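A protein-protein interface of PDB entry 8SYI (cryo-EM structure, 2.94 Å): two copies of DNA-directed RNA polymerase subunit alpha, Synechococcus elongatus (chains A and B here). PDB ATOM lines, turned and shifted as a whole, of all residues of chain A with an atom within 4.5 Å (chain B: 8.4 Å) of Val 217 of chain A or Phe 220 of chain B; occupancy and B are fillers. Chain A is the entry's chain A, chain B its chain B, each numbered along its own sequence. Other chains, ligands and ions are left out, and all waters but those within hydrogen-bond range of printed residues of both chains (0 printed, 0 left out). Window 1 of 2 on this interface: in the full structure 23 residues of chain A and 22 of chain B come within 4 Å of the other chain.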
ATOM      1  N   VAL A  35      -5.367  23.095  14.634  1.00  0.00           N
ATOM      2  CA  VAL A  35      -4.624  24.049  15.453  1.00  0.00           C
ATOM      3  C   VAL A  35      -5.277  24.197  16.820  1.00  0.00           C
ATOM      4  O   VAL A  35      -4.604  24.147  17.858  1.00  0.00           O
ATOM      5  CB  VAL A  35      -4.517  25.402  14.731  1.00  0.00           C
ATOM      6  CG1 VAL A  35      -3.926  26.448  15.650  1.00  0.00           C
ATOM      7  CG2 VAL A  35      -3.684  25.266  13.481  1.00  0.00           C
ATOM      8  N   ALA A  38      -4.861  20.932  18.987  1.00  0.00           N
ATOM      9  CA  ALA A  38      -3.483  20.788  19.434  1.00  0.00           C
ATOM     10  C   ALA A  38      -3.173  21.758  20.566  1.00  0.00           C
ATOM     11  O   ALA A  38      -2.573  21.374  21.580  1.00  0.00           O
ATOM     12  CB  ALA A  38      -2.529  21.002  18.263  1.00  0.00           C
ATOM     13  N   ALA A 213       2.790  27.122  22.267  1.00  0.00           N
ATOM     14  CA  ALA A 213       3.229  27.178  20.878  1.00  0.00           C
ATOM     15  C   ALA A 213       4.704  26.835  20.740  1.00  0.00           C
ATOM     16  O   ALA A 213       5.110  26.270  19.723  1.00  0.00           O
ATOM     17  CB  ALA A 213       2.951  28.557  20.288  1.00  0.00           C
ATOM     18  N   SER A 214       5.520  27.172  21.740  1.00  0.00           N
ATOM     19  CA  SER A 214       6.929  26.800  21.700  1.00  0.00           C
ATOM     20  C   SER A 214       7.139  25.311  21.936  1.00  0.00           C
ATOM     21  O   SER A 214       8.049  24.722  21.350  1.00  0.00           O
ATOM     22  CB  SER A 214       7.717  27.600  22.731  1.00  0.00           C
ATOM     23  OG  SER A 214       8.660  26.773  23.386  1.00  0.00           O
ATOM     24  N   CYS A 215       6.331  24.695  22.800  1.00  0.00           N
ATOM     25  CA  CYS A 215       6.425  23.249  22.978  1.00  0.00           C
ATOM     26  C   CYS A 215       6.032  22.496  21.712  1.00  0.00           C
ATOM     27  O   CYS A 215       6.679  21.504  21.356  1.00  0.00           O
ATOM     28  CB  CYS A 215       5.553  22.806  24.151  1.00  0.00           C
ATOM     29  SG  CYS A 215       5.049  21.076  24.107  1.00  0.00           S
ATOM     30  N   LEU A 216       4.986  22.950  21.019  1.00  0.00           N
ATOM     31  CA  LEU A 216       4.551  22.247  19.811  1.00  0.00           C
ATOM     32  C   LEU A 216       5.614  22.267  18.714  1.00  0.00           C
ATOM     33  O   LEU A 216       5.826  21.255  18.037  1.00  0.00           O
ATOM     34  CB  LEU A 216       3.246  22.846  19.291  1.00  0.00           C
ATOM     35  CG  LEU A 216       1.978  22.410  20.020  1.00  0.00           C
ATOM     36  CD1 LEU A 216       0.881  23.430  19.826  1.00  0.00           C
ATOM     37  CD2 LEU A 216       1.534  21.048  19.540  1.00  0.00           C
ATOM     38  N   VAL A 217       6.280  23.407  18.516  1.00  0.00           N
ATOM     39  CA  VAL A 217       7.307  23.501  17.481  1.00  0.00           C
ATOM     40  C   VAL A 217       8.457  22.550  17.779  1.00  0.00           C
ATOM     41  O   VAL A 217       8.948  21.849  16.888  1.00  0.00           O
ATOM     42  CB  VAL A 217       7.798  24.952  17.342  1.00  0.00           C
ATOM     43  CG1 VAL A 217       8.915  25.031  16.331  1.00  0.00           C
ATOM     44  CG2 VAL A 217       6.664  25.849  16.924  1.00  0.00           C
ATOM     45  N   ALA A 218       8.908  22.512  19.032  1.00  0.00           N
ATOM     46  CA  ALA A 218       9.938  21.560  19.425  1.00  0.00           C
ATOM     47  C   ALA A 218       9.469  20.119  19.311  1.00  0.00           C
ATOM     48  O   ALA A 218      10.307  19.221  19.190  1.00  0.00           O
ATOM     49  CB  ALA A 218      10.395  21.841  20.853  1.00  0.00           C
ATOM     50  N   LEU A 219       8.163  19.878  19.368  1.00  0.00           N
ATOM     51  CA  LEU A 219       7.625  18.546  19.126  1.00  0.00           C
ATOM     52  C   LEU A 219       7.639  18.152  17.653  1.00  0.00           C
ATOM     53  O   LEU A 219       7.902  16.989  17.338  1.00  0.00           O
ATOM     54  CB  LEU A 219       6.194  18.463  19.659  1.00  0.00           C
ATOM     55  CG  LEU A 219       5.674  17.107  20.120  1.00  0.00           C
ATOM     56  CD1 LEU A 219       6.626  16.479  21.111  1.00  0.00           C
ATOM     57  CD2 LEU A 219       4.303  17.285  20.739  1.00  0.00           C
ATOM     58  N   PHE A 220       7.359  19.088  16.745  1.00  0.00           N
ATOM     59  CA  PHE A 220       7.220  18.773  15.326  1.00  0.00           C
ATOM     60  C   PHE A 220       8.467  19.063  14.499  1.00  0.00           C
ATOM     61  O   PHE A 220       8.451  18.811  13.292  1.00  0.00           O
ATOM     62  CB  PHE A 220       6.040  19.545  14.722  1.00  0.00           C
ATOM     63  CG  PHE A 220       4.701  18.980  15.085  1.00  0.00           C
ATOM     64  CD1 PHE A 220       4.361  17.692  14.729  1.00  0.00           C
ATOM     65  CD2 PHE A 220       3.787  19.736  15.791  1.00  0.00           C
ATOM     66  CE1 PHE A 220       3.138  17.171  15.066  1.00  0.00           C
ATOM     67  CE2 PHE A 220       2.564  19.216  16.130  1.00  0.00           C
ATOM     68  CZ  PHE A 220       2.238  17.933  15.766  1.00  0.00           C
ATOM     69  N   GLU A 221       9.527  19.589  15.098  1.00  0.00           N
ATOM     70  CA  GLU A 221      10.729  19.946  14.348  1.00  0.00           C
ATOM     71  C   GLU A 221      11.650  18.759  14.055  1.00  0.00           C
ATOM     72  O   GLU A 221      12.248  18.718  12.974  1.00  0.00           O
ATOM     73  CB  GLU A 221      11.507  21.041  15.080  1.00  0.00           C
ATOM     74  CG  GLU A 221      12.716  21.546  14.316  1.00  0.00           C
ATOM     75  CD  GLU A 221      12.553  22.977  13.850  1.00  0.00           C
ATOM     76  OE1 GLU A 221      13.274  23.386  12.917  1.00  0.00           O
ATOM     77  OE2 GLU A 221      11.705  23.695  14.418  1.00  0.00           O
ATOM     78  N   PHE B   3      13.318  12.791  21.414  1.00  0.00           N
ATOM     79  CA  PHE B   3      12.813  11.509  20.952  1.00  0.00           C
ATOM     80  C   PHE B   3      13.502  11.140  19.647  1.00  0.00           C
ATOM     81  O   PHE B   3      14.118  11.978  18.985  1.00  0.00           O
ATOM     82  CB  PHE B   3      11.285  11.526  20.776  1.00  0.00           C
ATOM     83  CG  PHE B   3      10.790  12.503  19.740  1.00  0.00           C
ATOM     84  CD1 PHE B   3      10.758  12.164  18.398  1.00  0.00           C
ATOM     85  CD2 PHE B   3      10.336  13.752  20.115  1.00  0.00           C
ATOM     86  CE1 PHE B   3      10.300  13.055  17.455  1.00  0.00           C
ATOM     87  CE2 PHE B   3       9.876  14.645  19.173  1.00  0.00           C
ATOM     88  CZ  PHE B   3       9.856  14.295  17.842  1.00  0.00           C
ATOM     89  N   THR B  34      -1.897  13.560  20.230  1.00  0.00           N
ATOM     90  CA  THR B  34      -1.730  14.885  19.643  1.00  0.00           C
ATOM     91  C   THR B  34      -0.923  14.815  18.354  1.00  0.00           C
ATOM     92  O   THR B  34      -1.369  15.284  17.298  1.00  0.00           O
ATOM     93  CB  THR B  34      -1.044  15.815  20.644  1.00  0.00           C
ATOM     94  OG1 THR B  34      -1.793  15.855  21.862  1.00  0.00           O
ATOM     95  CG2 THR B  34      -0.930  17.215  20.085  1.00  0.00           C
ATOM     96  N   ALA B  38      -2.624  15.277  14.572  1.00  0.00           N
ATOM     97  CA  ALA B  38      -2.163  16.439  13.826  1.00  0.00           C
ATOM     98  C   ALA B  38      -1.451  16.034  12.544  1.00  0.00           C
ATOM     99  O   ALA B  38      -1.591  16.713  11.522  1.00  0.00           O
ATOM    100  CB  ALA B  38      -1.248  17.293  14.700  1.00  0.00           C
ATOM    101  N   VAL B  42      -3.188  16.684   8.425  1.00  0.00           N
ATOM    102  CA  VAL B  42      -2.405  17.424   7.443  1.00  0.00           C
ATOM    103  C   VAL B  42      -1.998  16.524   6.285  1.00  0.00           C
ATOM    104  O   VAL B  42      -2.046  16.934   5.120  1.00  0.00           O
ATOM    105  CB  VAL B  42      -1.184  18.068   8.120  1.00  0.00           C
ATOM    106  CG1 VAL B  42      -0.157  18.467   7.087  1.00  0.00           C
ATOM    107  CG2 VAL B  42      -1.610  19.272   8.927  1.00  0.00           C
ATOM    108  N   ALA B 212       4.572  17.292   5.712  1.00  0.00           N
ATOM    109  CA  ALA B 212       3.575  17.552   6.744  1.00  0.00           C
ATOM    110  C   ALA B 212       4.194  18.259   7.943  1.00  0.00           C
ATOM    111  O   ALA B 212       3.611  19.204   8.481  1.00  0.00           O
ATOM    112  CB  ALA B 212       2.910  16.247   7.176  1.00  0.00           C
ATOM    113  N   ALA B 213       5.380  17.820   8.373  1.00  0.00           N
ATOM    114  CA  ALA B 213       6.049  18.494   9.482  1.00  0.00           C
ATOM    115  C   ALA B 213       6.441  19.920   9.123  1.00  0.00           C
ATOM    116  O   ALA B 213       6.332  20.821   9.962  1.00  0.00           O
ATOM    117  CB  ALA B 213       7.276  17.701   9.919  1.00  0.00           C
ATOM    118  N   SER B 214       6.901  20.147   7.890  1.00  0.00           N
ATOM    119  CA  SER B 214       7.244  21.496   7.458  1.00  0.00           C
ATOM    120  C   SER B 214       6.024  22.405   7.455  1.00  0.00           C
ATOM    121  O   SER B 214       6.128  23.592   7.783  1.00  0.00           O
ATOM    122  CB  SER B 214       7.878  21.458   6.069  1.00  0.00           C
ATOM    123  OG  SER B 214       9.190  20.929   6.120  1.00  0.00           O
ATOM    124  N   CYS B 215       4.866  21.875   7.067  1.00  0.00           N
ATOM    125  CA  CYS B 215       3.654  22.687   7.076  1.00  0.00           C
ATOM    126  C   CYS B 215       3.114  22.900   8.485  1.00  0.00           C
ATOM    127  O   CYS B 215       2.476  23.924   8.748  1.00  0.00           O
ATOM    128  CB  CYS B 215       2.587  22.048   6.187  1.00  0.00           C
ATOM    129  SG  CYS B 215       0.975  21.839   6.965  1.00  0.00           S
ATOM    130  N   LEU B 216       3.351  21.953   9.396  1.00  0.00           N
ATOM    131  CA  LEU B 216       2.872  22.112  10.767  1.00  0.00           C
ATOM    132  C   LEU B 216       3.737  23.075  11.569  1.00  0.00           C
ATOM    133  O   LEU B 216       3.218  23.796  12.426  1.00  0.00           O
ATOM    134  CB  LEU B 216       2.814  20.759  11.466  1.00  0.00           C
ATOM    135  CG  LEU B 216       1.515  19.972  11.323  1.00  0.00           C
ATOM    136  CD1 LEU B 216       1.775  18.506  11.566  1.00  0.00           C
ATOM    137  CD2 LEU B 216       0.469  20.490  12.280  1.00  0.00           C
ATOM    138  N   VAL B 217       5.048  23.091  11.326  1.00  0.00           N
ATOM    139  CA  VAL B 217       5.927  23.986  12.075  1.00  0.00           C
ATOM    140  C   VAL B 217       5.574  25.443  11.802  1.00  0.00           C
ATOM    141  O   VAL B 217       5.571  26.278  12.716  1.00  0.00           O
ATOM    142  CB  VAL B 217       7.400  23.685  11.745  1.00  0.00           C
ATOM    143  CG1 VAL B 217       8.292  24.818  12.204  1.00  0.00           C
ATOM    144  CG2 VAL B 217       7.830  22.390  12.399  1.00  0.00           C
ATOM    145  N   ALA B 218       5.283  25.775  10.544  1.00  0.00           N
ATOM    146  CA  ALA B 218       4.987  27.149  10.164  1.00  0.00           C
ATOM    147  C   ALA B 218       3.611  27.614  10.619  1.00  0.00           C
ATOM    148  O   ALA B 218       3.344  28.818  10.575  1.00  0.00           O
ATOM    149  CB  ALA B 218       5.107  27.308   8.650  1.00  0.00           C
ATOM    150  N   LEU B 219       2.729  26.704  11.028  1.00  0.00           N
ATOM    151  CA  LEU B 219       1.454  27.101  11.614  1.00  0.00           C
ATOM    152  C   LEU B 219       1.603  27.554  13.060  1.00  0.00           C
ATOM    153  O   LEU B 219       0.946  28.511  13.478  1.00  0.00           O
ATOM    154  CB  LEU B 219       0.450  25.948  11.548  1.00  0.00           C
ATOM    155  CG  LEU B 219      -0.343  25.731  10.260  1.00  0.00           C
ATOM    156  CD1 LEU B 219      -1.045  24.389  10.312  1.00  0.00           C
ATOM    157  CD2 LEU B 219      -1.343  26.848  10.042  1.00  0.00           C
ATOM    158  N   PHE B 220       2.457  26.881  13.830  1.00  0.00           N
ATOM    159  CA  PHE B 220       2.605  27.164  15.251  1.00  0.00           C
ATOM    160  C   PHE B 220       3.736  28.130  15.555  1.00  0.00           C
ATOM    161  O   PHE B 220       3.764  28.694  16.652  1.00  0.00           O
ATOM    162  CB  PHE B 220       2.835  25.866  16.028  1.00  0.00           C
ATOM    163  CG  PHE B 220       1.671  24.923  15.988  1.00  0.00           C
ATOM    164  CD1 PHE B 220       0.479  25.249  16.604  1.00  0.00           C
ATOM    165  CD2 PHE B 220       1.767  23.713  15.328  1.00  0.00           C
ATOM    166  CE1 PHE B 220      -0.591  24.384  16.566  1.00  0.00           C
ATOM    167  CE2 PHE B 220       0.697  22.847  15.287  1.00  0.00           C
ATOM    168  CZ  PHE B 220      -0.481  23.183  15.906  1.00  0.00           C
ATOM    169  N   GLU B 221       4.668  28.332  14.628  1.00  0.00           N
ATOM    170  CA  GLU B 221       5.738  29.294  14.873  1.00  0.00           C
ATOM    171  C   GLU B 221       5.245  30.724  15.084  1.00  0.00           C
ATOM    172  O   GLU B 221       5.734  31.376  16.023  1.00  0.00           O
ATOM    173  CB  GLU B 221       6.762  29.224  13.734  1.00  0.00           C
ATOM    174  CG  GLU B 221       7.741  30.377  13.713  1.00  0.00           C
ATOM    175  CD  GLU B 221       8.983  30.093  14.529  1.00  0.00           C
ATOM    176  OE1 GLU B 221       9.457  31.010  15.230  1.00  0.00           O
ATOM    177  OE2 GLU B 221       9.484  28.952  14.470  1.00  0.00           O
ATOM    178  N   PRO B 222       4.318  31.274  14.289  1.00  0.00           N
ATOM    179  CA  PRO B 222       3.905  32.670  14.507  1.00  0.00           C
ATOM    180  C   PRO B 222       3.092  32.903  15.771  1.00  0.00           C
ATOM    181  O   PRO B 222       2.762  34.057  16.058  1.00  0.00           O
ATOM    182  CB  PRO B 222       3.064  32.983  13.261  1.00  0.00           C
ATOM    183  CG  PRO B 222       3.474  31.979  12.261  1.00  0.00           C
ATOM    184  CD  PRO B 222       3.733  30.746  13.047  1.00  0.00           C
ATOM    185  N   LEU B 223       2.741  31.865  16.527  1.00  0.00           N
ATOM    186  CA  LEU B 223       2.009  32.022  17.778  1.00  0.00           C
ATOM    187  C   LEU B 223       2.927  32.023  18.989  1.00  0.00           C
ATOM    188  O   LEU B 223       2.443  31.952  20.121  1.00  0.00           O
ATOM    189  CB  LEU B 223       0.964  30.916  17.926  1.00  0.00           C
ATOM    190  CG  LEU B 223      -0.179  30.901  16.916  1.00  0.00           C
ATOM    191  CD1 LEU B 223      -0.782  29.519  16.828  1.00  0.00           C
ATOM    192  CD2 LEU B 223      -1.230  31.909  17.312  1.00  0.00           C
ATOM    193  N   LYS B 224       4.235  32.101  18.777  1.00  0.00           N
ATOM    194  CA  LYS B 224       5.219  31.961  19.842  1.00  0.00           C
ATOM    195  C   LYS B 224       5.986  33.239  20.132  1.00  0.00           C
ATOM    196  O   LYS B 224       6.242  33.545  21.298  1.00  0.00           O
ATOM    197  CB  LYS B 224       6.207  30.846  19.485  1.00  0.00           C
ATOM    198  CG  LYS B 224       7.347  30.673  20.462  1.00  0.00           C
ATOM    199  CD  LYS B 224       8.657  30.457  19.732  1.00  0.00           C
ATOM    200  CE  LYS B 224       8.715  29.083  19.098  1.00  0.00           C
ATOM    201  NZ  LYS B 224      10.035  28.434  19.324  1.00  0.00           N
ATOM    202  N   ASN B 225       6.352  34.002  19.107  1.00  0.00           N
ATOM    203  CA  ASN B 225       7.204  35.171  19.276  1.00  0.00           C
ATOM    204  C   ASN B 225       6.426  36.473  19.406  1.00  0.00           C
ATOM    205  O   ASN B 225       7.045  37.535  19.517  1.00  0.00           O
ATOM    206  CB  ASN B 225       8.192  35.277  18.108  1.00  0.00           C
ATOM    207  CG  ASN B 225       7.512  35.604  16.794  1.00  0.00           C
ATOM    208  OD1 ASN B 225       7.451  36.764  16.387  1.00  0.00           O
ATOM    209  ND2 ASN B 225       7.003  34.581  16.120  1.00  0.00           N
ATOM    210  N   VAL B 226       5.096  36.429  19.390  1.00  0.00           N
ATOM    211  CA  VAL B 226       4.316  37.651  19.541  1.00  0.00           C
ATOM    212  C   VAL B 226       3.350  37.518  20.713  1.00  0.00           C
ATOM    213  O   VAL B 226       3.435  38.275  21.686  1.00  0.00           O
ATOM    214  CB  VAL B 226       3.574  38.007  18.238  1.00  0.00           C
ATOM    215  CG1 VAL B 226       4.512  38.728  17.284  1.00  0.00           C
ATOM    216  CG2 VAL B 226       3.016  36.766  17.573  1.00  0.00           C
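Val 217 of chain A touches just these residues of chain B: Phe 220 and Glu 221.
Of chain A, only Ala 38, Ala 213, Leu 216 and Val 217 come within 4 Å of Phe 220 of chain B.
Printed residues of chain B within 4 Å of Leu 216 of chain A: Phe 220 (3.7 Å).
Printed residues of chain A within 4 Å of Ala 38 of chain B: Phe 220.
Printed residues of chain A within 4 Å of Leu 216 of chain B: Phe 220.
Of the printed residues of chain A, Phe 3 of chain B touches Leu 219 (3.4 Å).
Printed residues of chain A within 4 Å of Ala 213 of chain B: Phe 220 (3.7 Å).
The nearest residue of chain A that does not touch Phe 220 of chain B is Val 35 of chain A (4.03 Å).
The nearest printed residue of chain B that does not touch Ala 213 of chain A is Lys 224 of chain B (4.1 Å).
Ala 213 of chain A touches Phe 220 of chain B, and with the chains exchanged Phe 220 of chain A touches Ala 213 of chain B.
Leu 216 of chain A touches Phe 220 of chain B, and with the chains exchanged Phe 220 of chain A touches Leu 216 of chain B.
Val 217 of chain A touches Phe 220 of chain B, and with the chains exchanged Phe 220 of chain A touches Val 217 of chain B.
Val 217 of chain A touches Glu 221 of chain B, but with the chains exchanged Glu 221 of chain A does not touch Val 217 of chain B (4.2 Å).
10 positions are printed for both chains.
O of Glu 221 of chain B is in hydrogen-bond range of ND2 of Asn 225 of chain B, 3.4 Å away.
CB of Ala 213 of chain A touches O of Phe 220 of chain B, at 3.7 Å.
CB of Ala 213 of chain A touches O of Leu 223 of chain B, at 3.4 Å.
Ser 214 of chain A touches Lys 224 of chain B.
Leu 216 of chain A touches Phe 220 of chain B (CD1 to CE1, 3.7 Å).
Val 217 of chain A touches Phe 220 of chain B.
Val 217 of chain A touches Glu 221 of chain B (CG2 to N, 3.9 Å).
Phe 3 of chain B touches Leu 219 of chain A.
Phe 220 of chain A touches Ala 38 of chain B (CZ to CB, 3.7 Å).
CD1 of Leu 216 of chain B touches CE1 of Phe 220 of chain A (3.99 Å).
Phe 220 of chain A touches Val 217 of chain B.
Hydrophobic or aromatic side chains of chain A within 4 Å of the printed part of chain B: Ala 38, Ala 213, Leu 216, Val 217 and Phe 220.
Hydrophobic or aromatic side chains of chain B within 4 Å of the printed part of chain A: Phe 3, Ala 38, Ala 213, Leu 216, Val 217, Phe 220 and Leu 223.
Among the printed residues, 12 pairs touch across the chains.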
